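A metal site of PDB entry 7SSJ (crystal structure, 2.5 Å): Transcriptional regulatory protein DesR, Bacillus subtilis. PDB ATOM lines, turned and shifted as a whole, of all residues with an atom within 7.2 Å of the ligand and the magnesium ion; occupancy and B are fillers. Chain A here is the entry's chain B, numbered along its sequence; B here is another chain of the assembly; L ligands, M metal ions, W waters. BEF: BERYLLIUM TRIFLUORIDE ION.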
ATOM      1  N   ALA A  11      -2.434 -16.895 -26.284  1.00  0.00           N
ATOM      2  CA  ALA A  11      -3.212 -15.760 -26.790  1.00  0.00           C
ATOM      3  C   ALA A  11      -3.479 -14.859 -25.602  1.00  0.00           C
ATOM      4  O   ALA A  11      -4.098 -15.277 -24.645  1.00  0.00           O
ATOM      5  CB  ALA A  11      -4.514 -16.230 -27.391  1.00  0.00           C
ATOM      6  N   GLU A  12      -2.936 -13.652 -25.643  1.00  0.00           N
ATOM      7  CA  GLU A  12      -3.086 -12.685 -24.569  1.00  0.00           C
ATOM      8  C   GLU A  12      -3.066 -11.320 -25.193  1.00  0.00           C
ATOM      9  O   GLU A  12      -2.129 -11.025 -25.923  1.00  0.00           O
ATOM     10  CB  GLU A  12      -1.884 -12.761 -23.617  1.00  0.00           C
ATOM     11  CG  GLU A  12      -2.263 -12.870 -22.169  1.00  0.00           C
ATOM     12  CD  GLU A  12      -2.800 -11.639 -21.473  1.00  0.00           C
ATOM     13  OE1 GLU A  12      -2.616 -11.531 -20.250  1.00  0.00           O
ATOM     14  OE2 GLU A  12      -3.414 -10.776 -22.138  1.00  0.00           O
ATOM     15  N   ASP A  13      -4.046 -10.452 -24.847  1.00  0.00           N
ATOM     16  CA  ASP A  13      -4.056  -9.092 -25.379  1.00  0.00           C
ATOM     17  C   ASP A  13      -3.024  -8.209 -24.729  1.00  0.00           C
ATOM     18  O   ASP A  13      -2.512  -7.293 -25.376  1.00  0.00           O
ATOM     19  CB  ASP A  13      -5.448  -8.452 -25.296  1.00  0.00           C
ATOM     20  CG  ASP A  13      -5.979  -8.242 -23.909  1.00  0.00           C
ATOM     21  OD1 ASP A  13      -5.970  -9.205 -23.108  1.00  0.00           O
ATOM     22  OD2 ASP A  13      -6.427  -7.105 -23.599  1.00  0.00           O
ATOM     23  N   GLN A  14      -2.712  -8.428 -23.445  1.00  0.00           N
ATOM     24  CA  GLN A  14      -1.717  -7.593 -22.738  1.00  0.00           C
ATOM     25  C   GLN A  14      -0.305  -7.990 -23.169  1.00  0.00           C
ATOM     26  O   GLN A  14       0.143  -9.094 -22.899  1.00  0.00           O
ATOM     27  CB  GLN A  14      -1.923  -7.683 -21.234  1.00  0.00           C
ATOM     28  CG  GLN A  14      -3.277  -7.160 -20.834  1.00  0.00           C
ATOM     29  CD  GLN A  14      -3.242  -5.718 -20.390  1.00  0.00           C
ATOM     30  OE1 GLN A  14      -2.217  -5.205 -19.938  1.00  0.00           O
ATOM     31  NE2 GLN A  14      -4.365  -5.040 -20.496  1.00  0.00           N
ATOM     32  N   LEU A  17       2.433  -8.983 -20.663  1.00  0.00           N
ATOM     33  CA  LEU A  17       1.995 -10.252 -20.091  1.00  0.00           C
ATOM     34  C   LEU A  17       2.239 -11.383 -21.037  1.00  0.00           C
ATOM     35  O   LEU A  17       2.665 -12.462 -20.612  1.00  0.00           O
ATOM     36  CB  LEU A  17       0.494 -10.158 -19.723  1.00  0.00           C
ATOM     37  CG  LEU A  17       0.152 -10.579 -18.303  1.00  0.00           C
ATOM     38  CD1 LEU A  17      -1.026  -9.835 -17.791  1.00  0.00           C
ATOM     39  CD2 LEU A  17      -0.059 -12.052 -18.246  1.00  0.00           C
ATOM     40  N   THR A  38      -2.550 -11.828 -29.894  1.00  0.00           N
ATOM     41  CA  THR A  38      -3.158 -10.800 -29.024  1.00  0.00           C
ATOM     42  C   THR A  38      -4.691 -10.781 -29.032  1.00  0.00           C
ATOM     43  O   THR A  38      -5.278  -9.984 -28.311  1.00  0.00           O
ATOM     44  CB  THR A  38      -2.590  -9.449 -29.360  1.00  0.00           C
ATOM     45  OG1 THR A  38      -2.781  -9.212 -30.768  1.00  0.00           O
ATOM     46  CG2 THR A  38      -1.136  -9.328 -28.979  1.00  0.00           C
ATOM     47  N   MET A  57      -5.005 -19.584 -23.283  1.00  0.00           N
ATOM     48  CA  MET A  57      -5.846 -18.517 -23.818  1.00  0.00           C
ATOM     49  C   MET A  57      -6.495 -17.571 -22.816  1.00  0.00           C
ATOM     50  O   MET A  57      -7.295 -17.976 -22.010  1.00  0.00           O
ATOM     51  CB  MET A  57      -6.935 -19.198 -24.661  1.00  0.00           C
ATOM     52  CG  MET A  57      -7.823 -18.251 -25.390  1.00  0.00           C
ATOM     53  SD  MET A  57      -7.888 -18.633 -27.144  1.00  0.00           S
ATOM     54  CE  MET A  57      -8.590 -20.279 -27.109  1.00  0.00           C
ATOM     55  N   ASP A  58      -6.247 -16.295 -22.978  1.00  0.00           N
ATOM     56  CA  ASP A  58      -6.886 -15.237 -22.183  1.00  0.00           C
ATOM     57  C   ASP A  58      -8.394 -15.155 -22.522  1.00  0.00           C
ATOM     58  O   ASP A  58      -8.800 -15.548 -23.633  1.00  0.00           O
ATOM     59  CB  ASP A  58      -6.241 -13.907 -22.542  1.00  0.00           C
ATOM     60  CG  ASP A  58      -6.771 -12.748 -21.758  1.00  0.00           C
ATOM     61  OD1 ASP A  58      -7.228 -12.982 -20.594  1.00  0.00           O
ATOM     62  OD2 ASP A  58      -6.744 -11.620 -22.282  1.00  0.00           O
ATOM     63  N   ILE A  59      -9.240 -14.638 -21.578  1.00  0.00           N
ATOM     64  CA  ILE A  59     -10.660 -14.470 -21.880  1.00  0.00           C
ATOM     65  C   ILE A  59     -10.862 -13.077 -22.563  1.00  0.00           C
ATOM     66  O   ILE A  59     -11.004 -12.987 -23.789  1.00  0.00           O
ATOM     67  CB  ILE A  59     -11.603 -14.748 -20.649  1.00  0.00           C
ATOM     68  CG1 ILE A  59     -11.813 -16.266 -20.434  1.00  0.00           C
ATOM     69  CG2 ILE A  59     -12.958 -14.023 -20.814  1.00  0.00           C
ATOM     70  CD1 ILE A  59     -12.596 -16.623 -19.148  1.00  0.00           C
ATOM     71  N   GLU A  60     -10.787 -12.009 -21.781  1.00  0.00           N
ATOM     72  CA  GLU A  60     -10.972 -10.663 -22.251  1.00  0.00           C
ATOM     73  C   GLU A  60      -9.850 -10.223 -23.184  1.00  0.00           C
ATOM     74  O   GLU A  60      -8.784  -9.794 -22.749  1.00  0.00           O
ATOM     75  CB  GLU A  60     -11.123  -9.717 -21.038  1.00  0.00           C
ATOM     76  CG  GLU A  60     -12.269 -10.110 -20.125  1.00  0.00           C
ATOM     77  CD  GLU A  60     -12.441  -9.306 -18.847  1.00  0.00           C
ATOM     78  OE1 GLU A  60     -13.326  -9.669 -18.042  1.00  0.00           O
ATOM     79  OE2 GLU A  60     -11.683  -8.336 -18.647  1.00  0.00           O
ATOM     80  N   MET A  61     -10.119 -10.308 -24.475  1.00  0.00           N
ATOM     81  CA  MET A  61      -9.228  -9.841 -25.533  1.00  0.00           C
ATOM     82  C   MET A  61     -10.065  -9.063 -26.549  1.00  0.00           C
ATOM     83  O   MET A  61     -11.078  -9.620 -27.006  1.00  0.00           O
ATOM     84  CB  MET A  61      -8.615 -11.043 -26.291  1.00  0.00           C
ATOM     85  CG  MET A  61      -7.744 -11.893 -25.452  1.00  0.00           C
ATOM     86  SD  MET A  61      -6.908 -13.075 -26.515  1.00  0.00           S
ATOM     87  CE  MET A  61      -7.984 -14.411 -26.509  1.00  0.00           C
ATOM     88  N   PRO A  62      -9.635  -7.863 -27.035  1.00  0.00           N
ATOM     89  CA  PRO A  62     -10.393  -7.175 -28.101  1.00  0.00           C
ATOM     90  C   PRO A  62     -10.482  -8.008 -29.374  1.00  0.00           C
ATOM     91  O   PRO A  62      -9.816  -9.043 -29.501  1.00  0.00           O
ATOM     92  CB  PRO A  62      -9.641  -5.860 -28.292  1.00  0.00           C
ATOM     93  CG  PRO A  62      -8.843  -5.687 -27.050  1.00  0.00           C
ATOM     94  CD  PRO A  62      -8.436  -7.084 -26.682  1.00  0.00           C
ATOM     95  N   GLY A  66     -11.441 -14.990 -25.860  1.00  0.00           N
ATOM     96  CA  GLY A  66     -10.961 -16.333 -25.652  1.00  0.00           C
ATOM     97  C   GLY A  66     -12.064 -17.356 -25.552  1.00  0.00           C
ATOM     98  O   GLY A  66     -11.892 -18.499 -25.972  1.00  0.00           O
ATOM     99  N   ILE A  82      -7.797 -22.095 -20.300  1.00  0.00           N
ATOM    100  CA  ILE A  82      -8.252 -20.719 -20.271  1.00  0.00           C
ATOM    101  C   ILE A  82      -7.667 -20.062 -19.066  1.00  0.00           C
ATOM    102  O   ILE A  82      -7.599 -20.659 -18.005  1.00  0.00           O
ATOM    103  CB  ILE A  82      -9.807 -20.687 -20.234  1.00  0.00           C
ATOM    104  CG1 ILE A  82     -10.424 -21.219 -21.530  1.00  0.00           C
ATOM    105  CG2 ILE A  82     -10.333 -19.303 -19.920  1.00  0.00           C
ATOM    106  CD1 ILE A  82      -9.970 -20.483 -22.770  1.00  0.00           C
ATOM    107  N   LEU A  83      -7.264 -18.832 -19.188  1.00  0.00           N
ATOM    108  CA  LEU A  83      -6.710 -18.060 -18.108  1.00  0.00           C
ATOM    109  C   LEU A  83      -7.514 -16.809 -18.040  1.00  0.00           C
ATOM    110  O   LEU A  83      -7.878 -16.276 -19.093  1.00  0.00           O
ATOM    111  CB  LEU A  83      -5.242 -17.674 -18.407  1.00  0.00           C
ATOM    112  CG  LEU A  83      -4.161 -18.781 -18.476  1.00  0.00           C
ATOM    113  CD1 LEU A  83      -2.797 -18.142 -18.592  1.00  0.00           C
ATOM    114  CD2 LEU A  83      -4.155 -19.607 -17.235  1.00  0.00           C
ATOM    115  N   THR A  84      -7.792 -16.296 -16.847  1.00  0.00           N
ATOM    116  CA  THR A  84      -8.545 -15.070 -16.657  1.00  0.00           C
ATOM    117  C   THR A  84      -8.164 -14.423 -15.368  1.00  0.00           C
ATOM    118  O   THR A  84      -7.626 -15.094 -14.496  1.00  0.00           O
ATOM    119  CB  THR A  84     -10.067 -15.297 -16.827  1.00  0.00           C
ATOM    120  OG1 THR A  84     -10.743 -14.015 -16.924  1.00  0.00           O
ATOM    121  CG2 THR A  84     -10.677 -16.204 -15.732  1.00  0.00           C
ATOM    122  N   THR A  85      -8.416 -13.139 -15.219  1.00  0.00           N
ATOM    123  CA  THR A  85      -8.000 -12.404 -14.033  1.00  0.00           C
ATOM    124  C   THR A  85      -9.083 -12.376 -12.972  1.00  0.00           C
ATOM    125  O   THR A  85      -8.794 -12.542 -11.794  1.00  0.00           O
ATOM    126  CB  THR A  85      -7.587 -10.981 -14.428  1.00  0.00           C
ATOM    127  OG1 THR A  85      -6.819 -11.035 -15.624  1.00  0.00           O
ATOM    128  CG2 THR A  85      -6.800 -10.275 -13.356  1.00  0.00           C
ATOM    129  N   PHE A  86     -10.328 -12.113 -13.403  1.00  0.00           N
ATOM    130  CA  PHE A  86     -11.491 -11.991 -12.533  1.00  0.00           C
ATOM    131  C   PHE A  86     -12.488 -13.038 -12.864  1.00  0.00           C
ATOM    132  O   PHE A  86     -12.777 -13.280 -14.036  1.00  0.00           O
ATOM    133  CB  PHE A  86     -12.160 -10.649 -12.750  1.00  0.00           C
ATOM    134  CG  PHE A  86     -11.318  -9.501 -12.300  1.00  0.00           C
ATOM    135  CD1 PHE A  86     -11.132  -9.242 -10.959  1.00  0.00           C
ATOM    136  CD2 PHE A  86     -10.697  -8.685 -13.218  1.00  0.00           C
ATOM    137  CE1 PHE A  86     -10.395  -8.152 -10.542  1.00  0.00           C
ATOM    138  CE2 PHE A  86      -9.938  -7.599 -12.811  1.00  0.00           C
ATOM    139  CZ  PHE A  86      -9.794  -7.331 -11.473  1.00  0.00           C
ATOM    140  N   ARG A  88     -15.975 -13.927 -13.455  1.00  0.00           N
ATOM    141  CA  ARG A  88     -17.150 -13.144 -13.826  1.00  0.00           C
ATOM    142  C   ARG A  88     -18.344 -14.036 -14.175  1.00  0.00           C
ATOM    143  O   ARG A  88     -18.163 -15.221 -14.535  1.00  0.00           O
ATOM    144  CB  ARG A  88     -16.815 -12.138 -14.936  1.00  0.00           C
ATOM    145  CG  ARG A  88     -15.831 -11.097 -14.459  1.00  0.00           C
ATOM    146  CD  ARG A  88     -15.651  -9.945 -15.403  1.00  0.00           C
ATOM    147  NE  ARG A  88     -15.273  -8.755 -14.647  1.00  0.00           N
ATOM    148  CZ  ARG A  88     -14.100  -8.148 -14.744  1.00  0.00           C
ATOM    149  NH1 ARG A  88     -13.180  -8.592 -15.600  1.00  0.00           N
ATOM    150  NH2 ARG A  88     -13.833  -7.076 -14.002  1.00  0.00           N
ATOM    151  N   TYR A  91     -18.747 -16.875 -17.144  1.00  0.00           N
ATOM    152  CA  TYR A  91     -17.449 -17.276 -17.695  1.00  0.00           C
ATOM    153  C   TYR A  91     -17.207 -18.742 -17.460  1.00  0.00           C
ATOM    154  O   TYR A  91     -16.860 -19.451 -18.402  1.00  0.00           O
ATOM    155  CB  TYR A  91     -16.294 -16.470 -17.075  1.00  0.00           C
ATOM    156  CG  TYR A  91     -16.064 -15.071 -17.609  1.00  0.00           C
ATOM    157  CD1 TYR A  91     -16.736 -14.610 -18.728  1.00  0.00           C
ATOM    158  CD2 TYR A  91     -15.104 -14.239 -17.029  1.00  0.00           C
ATOM    159  CE1 TYR A  91     -16.513 -13.336 -19.232  1.00  0.00           C
ATOM    160  CE2 TYR A  91     -14.865 -12.962 -17.539  1.00  0.00           C
ATOM    161  CZ  TYR A  91     -15.592 -12.505 -18.610  1.00  0.00           C
ATOM    162  OH  TYR A  91     -15.358 -11.234 -19.089  1.00  0.00           O
ATOM    163  N   LYS A 106      -4.872 -16.179 -14.003  1.00  0.00           N
ATOM    164  CA  LYS A 106      -3.685 -15.730 -14.721  1.00  0.00           C
ATOM    165  C   LYS A 106      -2.420 -15.582 -13.863  1.00  0.00           C
ATOM    166  O   LYS A 106      -1.320 -15.959 -14.328  1.00  0.00           O
ATOM    167  CB  LYS A 106      -3.958 -14.410 -15.438  1.00  0.00           C
ATOM    168  CG  LYS A 106      -3.060 -14.230 -16.640  1.00  0.00           C
ATOM    169  CD  LYS A 106      -3.576 -13.106 -17.465  1.00  0.00           C
ATOM    170  CE  LYS A 106      -4.620 -13.633 -18.383  1.00  0.00           C
ATOM    171  NZ  LYS A 106      -4.968 -12.572 -19.319  1.00  0.00           N
ATOM    172  N   ASP B  43     -10.273  -3.015 -12.983  1.00  0.00           N
ATOM    173  CA  ASP B  43     -10.114  -4.003 -14.033  1.00  0.00           C
ATOM    174  C   ASP B  43      -8.662  -4.042 -14.550  1.00  0.00           C
ATOM    175  O   ASP B  43      -8.107  -5.138 -14.738  1.00  0.00           O
ATOM    176  CB  ASP B  43     -11.090  -3.744 -15.163  1.00  0.00           C
ATOM    177  CG  ASP B  43     -11.306  -4.986 -16.010  1.00  0.00           C
ATOM    178  OD1 ASP B  43     -10.285  -5.550 -16.523  1.00  0.00           O
ATOM    179  OD2 ASP B  43     -12.466  -5.409 -16.141  1.00  0.00           O
ATOM    180  N   GLN B  47      -4.989  -6.645 -14.291  1.00  0.00           N
ATOM    181  CA  GLN B  47      -4.034  -6.964 -15.364  1.00  0.00           C
ATOM    182  C   GLN B  47      -2.610  -6.562 -14.940  1.00  0.00           C
ATOM    183  O   GLN B  47      -1.661  -7.325 -15.161  1.00  0.00           O
ATOM    184  CB  GLN B  47      -4.431  -6.220 -16.635  1.00  0.00           C
ATOM    185  CG  GLN B  47      -5.882  -6.410 -17.068  1.00  0.00           C
ATOM    186  CD  GLN B  47      -6.216  -7.820 -17.494  1.00  0.00           C
ATOM    187  OE1 GLN B  47      -5.396  -8.487 -18.136  1.00  0.00           O
ATOM    188  NE2 GLN B  47      -7.422  -8.328 -17.162  1.00  0.00           N
ATOM    189  N   SER B  50      -1.363  -8.904 -12.153  1.00  0.00           N
ATOM    190  CA  SER B  50      -1.030 -10.201 -12.743  1.00  0.00           C
ATOM    191  C   SER B  50       0.334 -10.104 -13.434  1.00  0.00           C
ATOM    192  O   SER B  50       1.163 -10.994 -13.306  1.00  0.00           O
ATOM    193  CB  SER B  50      -2.093 -10.617 -13.760  1.00  0.00           C
ATOM    194  OG  SER B  50      -3.357 -10.853 -13.153  1.00  0.00           O
ATOM    195  N   ASN B 202      -2.633  -0.382 -21.993  1.00  0.00           N
ATOM    196  CA  ASN B 202      -2.281  -1.350 -23.058  1.00  0.00           C
ATOM    197  C   ASN B 202      -2.335  -0.721 -24.489  1.00  0.00           C
ATOM    198  O   ASN B 202      -2.452  -1.423 -25.500  1.00  0.00           O
ATOM    199  CB  ASN B 202      -3.100  -2.639 -22.967  1.00  0.00           C
ATOM    200  CG  ASN B 202      -2.466  -3.830 -23.685  1.00  0.00           C
ATOM    201  OD1 ASN B 202      -1.245  -3.990 -23.785  1.00  0.00           O
ATOM    202  ND2 ASN B 202      -3.278  -4.697 -24.206  1.00  0.00           N
ATOM    203  N   SER B 223     -14.110  -5.515 -23.937  1.00  0.00           N
ATOM    204  CA  SER B 223     -14.657  -6.854 -24.128  1.00  0.00           C
ATOM    205  C   SER B 223     -13.576  -7.866 -24.497  1.00  0.00           C
ATOM    206  O   SER B 223     -12.517  -7.849 -23.881  1.00  0.00           O
ATOM    207  CB  SER B 223     -15.834  -6.841 -25.111  1.00  0.00           C
ATOM    208  OG  SER B 223     -16.733  -7.910 -24.868  1.00  0.00           O
HETATM  209 BE   BEF L   1      -8.069 -12.120 -19.510  1.00  0.00          BE
HETATM  210  F1  BEF L   1      -9.485 -12.766 -19.387  1.00  0.00           F
HETATM  211  F2  BEF L   1      -7.470 -12.247 -18.099  1.00  0.00           F
HETATM  212  F3  BEF L   1      -8.108 -10.579 -19.717  1.00  0.00           F
HETATM  213 MG    MG M   1      -7.067  -9.831 -21.398  1.00  0.00          MG
HETATM  214  O   HOH W   1      -7.407  -7.833 -21.038  1.00  0.00           O
HETATM  215  O   HOH W   2      -5.389  -9.702 -20.120  1.00  0.00           O
HETATM  216  O   HOH W   3     -10.889 -11.494 -16.601  1.00  0.00           O
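OD1 of Asp 58 binds BE of the ligand (1.6 Å).
F2 of the ligand is in hydrogen-bond range of N of Thr 85, 3.2 Å away.
A fluorine (F2) of the ligand is in hydrogen-bond range of the side-chain amino group (NZ) of Lys 106 (2.8 Å).
OG1 of Thr 84 sits at hydrogen-bond distance from F1 of the ligand, 3.0 Å away.
The backbone NH of Glu 60 lies within hydrogen-bond range of a fluorine (F1) of the ligand, at 2.8 Å.
N of Ile 59 lies within hydrogen-bond range of F1 of the ligand (2.9 Å).
A fluorine (F3) of the ligand sits close to the side-chain amide nitrogen (NE2) of Gln 47 of chain B, at 3.5 Å.
OG1 of Thr 85 lies within hydrogen-bond range of F2 of the ligand, 2.8 Å away.
The backbone carbonyl oxygen (O) of Asp 58 sits close to the backbone NH (N) of Gly 66, 3.5 Å away.
O of Asp 13 sits at hydrogen-bond distance from ND2 of Asn 202 of chain B.
The side-chain amide nitrogen (NE2) of Gln 47 of chain B sits at hydrogen-bond distance from the side-chain hydroxyl (OG1) of Thr 85, 3.2 Å away.
The backbone NH (N) of Leu 83 is in hydrogen-bond range of the backbone carbonyl oxygen (O) of Met 57 (2.9 Å).
N of Asp 58 is in hydrogen-bond range of O of Ala 11 (2.9 Å).
The side-chain carboxylate (OE1) of Glu 12 is in salt-bridge range of the side-chain amino group (NZ) of Lys 106.
The backbone carbonyl oxygen (O) of Leu 83 is in hydrogen-bond range of the backbone NH (N) of Ile 59 (3.3 Å).
OE2 of Glu 12 sits at hydrogen-bond distance from N of Gln 14, 2.8 Å away.
O of Leu 83 touches F1 of the ligand, at 3.9 Å.
Hydrophobic or aromatic side chains that line the ligand: Ile 59.
Of the 26 residues printed, 8 come within 4 Å of the ligand.
Glu 12 touches the magnesium ion (OE2 to MG, 3.8 Å).
Gln 47 of chain B touches the magnesium ion (OE1 to MG, 3.9 Å).
Of the 26 residues printed, 5 come within 4 Å of the magnesium ion.
The nearest printed residue that does not touch the magnesium ion is Lys 106 (4.03 Å).
OD2 of Asp 58 is bound to the magnesium ion, at 2.0 Å.
The magnesium ion is bound by water W1 (2.1 Å).
Water W2 binds the magnesium ion.
F3 of the ligand is bound to the magnesium ion.
The magnesium ion is bound by OD1 of Asp 13.
O of Glu 60 binds the magnesium ion, at 2.2 Å.
The magnesium ion has six donor atoms within binding distance.
Water W2 bridges the side-chain amino group of Lys 106 (3.0 Å) and the side-chain carboxylate of Glu 12 (3.0 Å).
Water W3 lies within hydrogen-bond range of OG1 of Thr 84 (2.5 Å), N of Thr 85 (3.3 Å), N of Phe 86 (3.3 Å), OE1 of Glu 60 (3.4 Å) and F1 of the ligand (3.4 Å).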
